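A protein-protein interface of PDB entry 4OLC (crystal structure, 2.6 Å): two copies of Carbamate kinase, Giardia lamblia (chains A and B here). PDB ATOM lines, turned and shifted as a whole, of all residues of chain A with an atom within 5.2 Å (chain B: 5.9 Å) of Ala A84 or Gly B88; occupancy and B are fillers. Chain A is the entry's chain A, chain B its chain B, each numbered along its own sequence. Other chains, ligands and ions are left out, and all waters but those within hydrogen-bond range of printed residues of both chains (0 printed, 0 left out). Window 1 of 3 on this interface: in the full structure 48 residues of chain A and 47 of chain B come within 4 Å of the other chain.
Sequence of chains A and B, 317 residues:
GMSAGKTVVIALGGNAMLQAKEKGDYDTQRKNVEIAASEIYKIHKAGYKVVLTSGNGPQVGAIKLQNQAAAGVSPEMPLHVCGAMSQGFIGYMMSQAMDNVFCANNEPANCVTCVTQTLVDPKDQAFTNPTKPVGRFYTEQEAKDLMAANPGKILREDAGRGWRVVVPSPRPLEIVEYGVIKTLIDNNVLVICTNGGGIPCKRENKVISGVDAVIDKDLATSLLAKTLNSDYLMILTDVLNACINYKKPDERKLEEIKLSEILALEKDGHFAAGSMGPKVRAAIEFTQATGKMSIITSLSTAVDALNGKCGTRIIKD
NE2 of Gln A87 lies close to N of Ile A199, 3.2 Å away.
Printed residues of chain A that touch a printed residue of chain B: His A80, Val A81, Ala A84, Met A85, Gly A88 and Ile A199.
Along chain A the printed residues that touch a printed residue of chain B span positions 80 to 199.
Of the 12 printed residues of chain B, 6 touch a printed residue of chain A.
Hydrophobic or aromatic side chains of chain B that line the printed part of chain A: Ala B84, Met B85, Phe B89, Tyr B92 and Val B115.
Among the printed residues, 9 pairs touch across the chains.
Among the printed residues, no Asp or Glu carboxylate lies within 4 Å of a Lys or Arg side-chain nitrogen of the other chain.
Of the printed residues of chain B, His A80 touches Tyr B92.
Cys A82 touches none of the printed residues of chain B.
Of chain B, only Gly B88 (3.3 Å) and Tyr B92 (3.6 Å) come within 4 Å of Ala A84.
Printed residues of chain B within 4 Å of Ile A199: Tyr B92 (3.5 Å).
Printed residues of chain A within 4 Å of Ala B84: Gly A88.
Of the printed residues of chain A, Met B85 touches Met A85.
Of chain A, only Ala A84 comes within 4 Å of Gly B88.
Of the printed residues of chain A, Phe B89 touches Val A81 and Met A85.
Met B93 touches none of the printed residues of chain A.
The nearest printed residue of chain A that does not touch Gly B88 is Val A115 (4.1 Å).
The nearest printed residue of chain A that does not touch Tyr B92 is Val A115 (4.2 Å).
The side-chain hydroxyl (OH) of Tyr B92 is in hydrogen-bond range of a ring nitrogen (ND1) of His A80, 3.1 Å away.
CG1 of Val A81 touches CD1 of Phe B89, at 3.4 Å.
Ala A84 touches Gly B88.
Tyr B92 touches Ala A84.
Met B85 touches Met A85.
Met A85 touches Phe B89.
O of Gly A88 touches CB of Ala B84 (3.6 Å).
CA of Gly A88 touches CG2 of Val B115, at 3.96 Å.
Tyr B92 touches Ile A199.
Ala A84 touches Gly B88, and with the chains exchanged Gly A88 touches Ala B84.
Met B85 touches its own counterpart, Met A85.
Gly A88 touches Val B115, but with the chains exchanged Val A115 does not touch Gly B88 (4.1 Å).
Positions printed for both chains: 83, 84, 85, 86, 87, 88 and 115.
Of the 9 pairs that touch across the chains among the printed residues, 3 have their exchanged pair printed and touching as well.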
ATOM      1  N   LEU A  79      31.476   5.944   6.675  1.00  0.00           N
ATOM      2  CA  LEU A  79      31.802   6.057   5.253  1.00  0.00           C
ATOM      3  C   LEU A  79      30.660   6.680   4.445  1.00  0.00           C
ATOM      4  O   LEU A  79      30.899   7.568   3.627  1.00  0.00           O
ATOM      5  CB  LEU A  79      32.193   4.689   4.686  1.00  0.00           C
ATOM      6  CG  LEU A  79      32.742   4.586   3.260  1.00  0.00           C
ATOM      7  CD1 LEU A  79      33.996   5.433   3.068  1.00  0.00           C
ATOM      8  CD2 LEU A  79      33.008   3.128   2.868  1.00  0.00           C
ATOM      9  N   HIS A  80      29.427   6.222   4.690  1.00  0.00           N
ATOM     10  CA  HIS A  80      28.258   6.718   3.963  1.00  0.00           C
ATOM     11  C   HIS A  80      28.065   8.227   4.128  1.00  0.00           C
ATOM     12  O   HIS A  80      27.831   8.916   3.147  1.00  0.00           O
ATOM     13  CB  HIS A  80      26.975   5.905   4.259  1.00  0.00           C
ATOM     14  CG  HIS A  80      26.493   5.986   5.677  1.00  0.00           C
ATOM     15  ND1 HIS A  80      25.474   6.830   6.073  1.00  0.00           N
ATOM     16  CD2 HIS A  80      26.871   5.313   6.793  1.00  0.00           C
ATOM     17  CE1 HIS A  80      25.256   6.683   7.362  1.00  0.00           C
ATOM     18  NE2 HIS A  80      26.091   5.771   7.831  1.00  0.00           N
ATOM     19  N   VAL A  81      28.202   8.746   5.347  1.00  0.00           N
ATOM     20  CA  VAL A  81      28.232  10.197   5.577  1.00  0.00           C
ATOM     21  C   VAL A  81      29.360  10.914   4.822  1.00  0.00           C
ATOM     22  O   VAL A  81      29.183  12.042   4.359  1.00  0.00           O
ATOM     23  CB  VAL A  81      28.331  10.521   7.095  1.00  0.00           C
ATOM     24  CG1 VAL A  81      28.545  12.016   7.341  1.00  0.00           C
ATOM     25  CG2 VAL A  81      27.078  10.024   7.812  1.00  0.00           C
ATOM     26  N   CYS A  82      30.514  10.254   4.705  1.00  0.00           N
ATOM     27  CA  CYS A  82      31.698  10.838   4.086  1.00  0.00           C
ATOM     28  C   CYS A  82      31.474  10.955   2.597  1.00  0.00           C
ATOM     29  O   CYS A  82      31.941  11.896   1.943  1.00  0.00           O
ATOM     30  CB  CYS A  82      32.935   9.962   4.353  1.00  0.00           C
ATOM     31  SG  CYS A  82      33.645  10.089   6.005  1.00  0.00           S
ATOM     32  N   GLY A  83      30.773   9.965   2.058  1.00  0.00           N
ATOM     33  CA  GLY A  83      30.267  10.019   0.690  1.00  0.00           C
ATOM     34  C   GLY A  83      29.347  11.208   0.432  1.00  0.00           C
ATOM     35  O   GLY A  83      29.558  11.955  -0.524  1.00  0.00           O
ATOM     36  N   ALA A  84      28.341  11.399   1.284  1.00  0.00           N
ATOM     37  CA  ALA A  84      27.463  12.552   1.170  1.00  0.00           C
ATOM     38  C   ALA A  84      28.243  13.864   1.180  1.00  0.00           C
ATOM     39  O   ALA A  84      27.931  14.782   0.407  1.00  0.00           O
ATOM     40  CB  ALA A  84      26.423  12.542   2.274  1.00  0.00           C
ATOM     41  N   MET A  85      29.247  13.963   2.050  1.00  0.00           N
ATOM     42  CA  MET A  85      30.094  15.150   2.079  1.00  0.00           C
ATOM     43  C   MET A  85      30.856  15.337   0.778  1.00  0.00           C
ATOM     44  O   MET A  85      31.105  16.470   0.375  1.00  0.00           O
ATOM     45  CB  MET A  85      31.081  15.114   3.241  1.00  0.00           C
ATOM     46  CG  MET A  85      30.439  15.231   4.578  1.00  0.00           C
ATOM     47  SD  MET A  85      31.691  15.114   5.878  1.00  0.00           S
ATOM     48  CE  MET A  85      30.670  15.360   7.327  1.00  0.00           C
ATOM     49  N   SER A  86      31.236  14.239   0.125  1.00  0.00           N
ATOM     50  CA  SER A  86      31.990  14.346  -1.128  1.00  0.00           C
ATOM     51  C   SER A  86      31.065  14.747  -2.271  1.00  0.00           C
ATOM     52  O   SER A  86      31.462  15.494  -3.153  1.00  0.00           O
ATOM     53  CB  SER A  86      32.731  13.052  -1.465  1.00  0.00           C
ATOM     54  OG  SER A  86      31.836  11.998  -1.782  1.00  0.00           O
ATOM     55  N   GLN A  87      29.831  14.247  -2.235  1.00  0.00           N
ATOM     56  CA  GLN A  87      28.791  14.686  -3.155  1.00  0.00           C
ATOM     57  C   GLN A  87      28.591  16.190  -3.091  1.00  0.00           C
ATOM     58  O   GLN A  87      28.456  16.835  -4.124  1.00  0.00           O
ATOM     59  CB  GLN A  87      27.455  14.003  -2.851  1.00  0.00           C
ATOM     60  CG  GLN A  87      27.324  12.592  -3.375  1.00  0.00           C
ATOM     61  CD  GLN A  87      25.879  12.124  -3.361  1.00  0.00           C
ATOM     62  OE1 GLN A  87      24.949  12.919  -3.154  1.00  0.00           O
ATOM     63  NE2 GLN A  87      25.676  10.833  -3.583  1.00  0.00           N
ATOM     64  N   GLY A  88      28.549  16.748  -1.883  1.00  0.00           N
ATOM     65  CA  GLY A  88      28.432  18.186  -1.724  1.00  0.00           C
ATOM     66  C   GLY A  88      29.609  18.959  -2.315  1.00  0.00           C
ATOM     67  O   GLY A  88      29.416  20.039  -2.875  1.00  0.00           O
ATOM     68  N   VAL A 115      21.996  16.064  -4.001  1.00  0.00           N
ATOM     69  CA  VAL A 115      22.480  14.996  -3.147  1.00  0.00           C
ATOM     70  C   VAL A 115      21.706  13.719  -3.494  1.00  0.00           C
ATOM     71  O   VAL A 115      20.489  13.728  -3.540  1.00  0.00           O
ATOM     72  CB  VAL A 115      22.303  15.330  -1.638  1.00  0.00           C
ATOM     73  CG1 VAL A 115      22.538  14.092  -0.792  1.00  0.00           C
ATOM     74  CG2 VAL A 115      23.227  16.452  -1.208  1.00  0.00           C
ATOM     75  N   ILE A 199      25.213   7.939  -2.335  1.00  0.00           N
ATOM     76  CA  ILE A 199      25.415   7.454  -0.986  1.00  0.00           C
ATOM     77  C   ILE A 199      24.725   6.094  -0.872  1.00  0.00           C
ATOM     78  O   ILE A 199      23.511   5.994  -1.038  1.00  0.00           O
ATOM     79  CB  ILE A 199      24.801   8.432   0.026  1.00  0.00           C
ATOM     80  CG1 ILE A 199      25.460   9.803  -0.110  1.00  0.00           C
ATOM     81  CG2 ILE A 199      24.893   7.888   1.451  1.00  0.00           C
ATOM     82  CD1 ILE A 199      24.464  10.950  -0.037  1.00  0.00           C
ATOM     83  N   GLY B  83      31.795  24.374   3.895  1.00  0.00           N
ATOM     84  CA  GLY B  83      30.371  24.644   3.715  1.00  0.00           C
ATOM     85  C   GLY B  83      29.681  23.680   2.759  1.00  0.00           C
ATOM     86  O   GLY B  83      28.722  23.016   3.154  1.00  0.00           O
ATOM     87  N   ALA B  84      30.189  23.585   1.524  1.00  0.00           N
ATOM     88  CA  ALA B  84      29.747  22.585   0.544  1.00  0.00           C
ATOM     89  C   ALA B  84      29.592  21.186   1.145  1.00  0.00           C
ATOM     90  O   ALA B  84      28.534  20.574   1.024  1.00  0.00           O
ATOM     91  CB  ALA B  84      30.714  22.540  -0.646  1.00  0.00           C
ATOM     92  N   MET B  85      30.640  20.673   1.790  1.00  0.00           N
ATOM     93  CA  MET B  85      30.536  19.396   2.493  1.00  0.00           C
ATOM     94  C   MET B  85      29.420  19.347   3.558  1.00  0.00           C
ATOM     95  O   MET B  85      28.792  18.299   3.746  1.00  0.00           O
ATOM     96  CB  MET B  85      31.871  19.021   3.120  1.00  0.00           C
ATOM     97  CG  MET B  85      32.962  18.690   2.111  1.00  0.00           C
ATOM     98  SD  MET B  85      34.592  18.437   2.867  1.00  0.00           S
ATOM     99  CE  MET B  85      35.628  18.445   1.409  1.00  0.00           C
ATOM    100  N   SER B  86      29.163  20.467   4.247  1.00  0.00           N
ATOM    101  CA  SER B  86      28.124  20.491   5.286  1.00  0.00           C
ATOM    102  C   SER B  86      26.730  20.338   4.670  1.00  0.00           C
ATOM    103  O   SER B  86      25.816  19.745   5.265  1.00  0.00           O
ATOM    104  CB  SER B  86      28.194  21.771   6.140  1.00  0.00           C
ATOM    105  OG  SER B  86      27.819  22.945   5.434  1.00  0.00           O
ATOM    106  N   GLN B  87      26.572  20.885   3.470  1.00  0.00           N
ATOM    107  CA  GLN B  87      25.325  20.762   2.756  1.00  0.00           C
ATOM    108  C   GLN B  87      25.127  19.311   2.361  1.00  0.00           C
ATOM    109  O   GLN B  87      24.015  18.784   2.487  1.00  0.00           O
ATOM    110  CB  GLN B  87      25.306  21.668   1.529  1.00  0.00           C
ATOM    111  CG  GLN B  87      25.114  23.133   1.840  1.00  0.00           C
ATOM    112  CD  GLN B  87      25.102  23.943   0.566  1.00  0.00           C
ATOM    113  OE1 GLN B  87      25.118  23.376  -0.519  1.00  0.00           O
ATOM    114  NE2 GLN B  87      25.098  25.260   0.685  1.00  0.00           N
ATOM    115  N   GLY B  88      26.196  18.672   1.885  1.00  0.00           N
ATOM    116  CA  GLY B  88      26.128  17.272   1.504  1.00  0.00           C
ATOM    117  C   GLY B  88      25.642  16.440   2.670  1.00  0.00           C
ATOM    118  O   GLY B  88      24.693  15.661   2.558  1.00  0.00           O
ATOM    119  N   PHE B  89      26.299  16.637   3.806  1.00  0.00           N
ATOM    120  CA  PHE B  89      25.976  15.972   5.058  1.00  0.00           C
ATOM    121  C   PHE B  89      24.558  16.304   5.584  1.00  0.00           C
ATOM    122  O   PHE B  89      23.730  15.404   5.789  1.00  0.00           O
ATOM    123  CB  PHE B  89      27.028  16.365   6.093  1.00  0.00           C
ATOM    124  CG  PHE B  89      26.818  15.745   7.450  1.00  0.00           C
ATOM    125  CD1 PHE B  89      26.226  14.504   7.587  1.00  0.00           C
ATOM    126  CD2 PHE B  89      27.231  16.410   8.593  1.00  0.00           C
ATOM    127  CE1 PHE B  89      26.047  13.939   8.838  1.00  0.00           C
ATOM    128  CE2 PHE B  89      27.052  15.848   9.842  1.00  0.00           C
ATOM    129  CZ  PHE B  89      26.454  14.610   9.962  1.00  0.00           C
ATOM    130  N   ILE B  90      24.294  17.587   5.825  1.00  0.00           N
ATOM    131  CA  ILE B  90      23.010  18.003   6.357  1.00  0.00           C
ATOM    132  C   ILE B  90      21.875  17.642   5.401  1.00  0.00           C
ATOM    133  O   ILE B  90      20.849  17.067   5.808  1.00  0.00           O
ATOM    134  CB  ILE B  90      22.992  19.500   6.638  1.00  0.00           C
ATOM    135  CG1 ILE B  90      24.067  19.849   7.673  1.00  0.00           C
ATOM    136  CG2 ILE B  90      21.621  19.928   7.152  1.00  0.00           C
ATOM    137  CD1 ILE B  90      24.586  21.279   7.566  1.00  0.00           C
ATOM    138  N   GLY B  91      22.066  17.984   4.128  1.00  0.00           N
ATOM    139  CA  GLY B  91      21.099  17.687   3.097  1.00  0.00           C
ATOM    140  C   GLY B  91      20.856  16.203   2.993  1.00  0.00           C
ATOM    141  O   GLY B  91      19.796  15.764   2.595  1.00  0.00           O
ATOM    142  N   TYR B  92      21.850  15.416   3.361  1.00  0.00           N
ATOM    143  CA  TYR B  92      21.704  13.968   3.301  1.00  0.00           C
ATOM    144  C   TYR B  92      20.796  13.423   4.426  1.00  0.00           C
ATOM    145  O   TYR B  92      19.981  12.534   4.199  1.00  0.00           O
ATOM    146  CB  TYR B  92      23.087  13.290   3.287  1.00  0.00           C
ATOM    147  CG  TYR B  92      23.055  11.808   3.613  1.00  0.00           C
ATOM    148  CD1 TYR B  92      22.277  10.925   2.864  1.00  0.00           C
ATOM    149  CD2 TYR B  92      23.807  11.293   4.670  1.00  0.00           C
ATOM    150  CE1 TYR B  92      22.246   9.576   3.163  1.00  0.00           C
ATOM    151  CE2 TYR B  92      23.797   9.951   4.969  1.00  0.00           C
ATOM    152  CZ  TYR B  92      23.019   9.091   4.213  1.00  0.00           C
ATOM    153  OH  TYR B  92      23.011   7.748   4.512  1.00  0.00           O
ATOM    154  N   MET B  93      20.956  13.944   5.642  1.00  0.00           N
ATOM    155  CA  MET B  93      20.177  13.488   6.796  1.00  0.00           C
ATOM    156  C   MET B  93      18.736  13.933   6.641  1.00  0.00           C
ATOM    157  O   MET B  93      17.792  13.164   6.840  1.00  0.00           O
ATOM    158  CB  MET B  93      20.765  14.047   8.096  1.00  0.00           C
ATOM    159  CG  MET B  93      22.122  13.457   8.463  1.00  0.00           C
ATOM    160  SD  MET B  93      22.733  14.027  10.063  1.00  0.00           S
ATOM    161  CE  MET B  93      22.945  15.777   9.750  1.00  0.00           C
ATOM    162  N   VAL B 115      22.568  21.252  -3.662  1.00  0.00           N
ATOM    163  CA  VAL B 115      23.740  22.018  -3.266  1.00  0.00           C
ATOM    164  C   VAL B 115      23.444  23.448  -3.699  1.00  0.00           C
ATOM    165  O   VAL B 115      22.818  23.670  -4.740  1.00  0.00           O
ATOM    166  CB  VAL B 115      25.039  21.456  -3.912  1.00  0.00           C
ATOM    167  CG1 VAL B 115      26.218  22.399  -3.724  1.00  0.00           C
ATOM    168  CG2 VAL B 115      25.354  20.077  -3.344  1.00  0.00           C
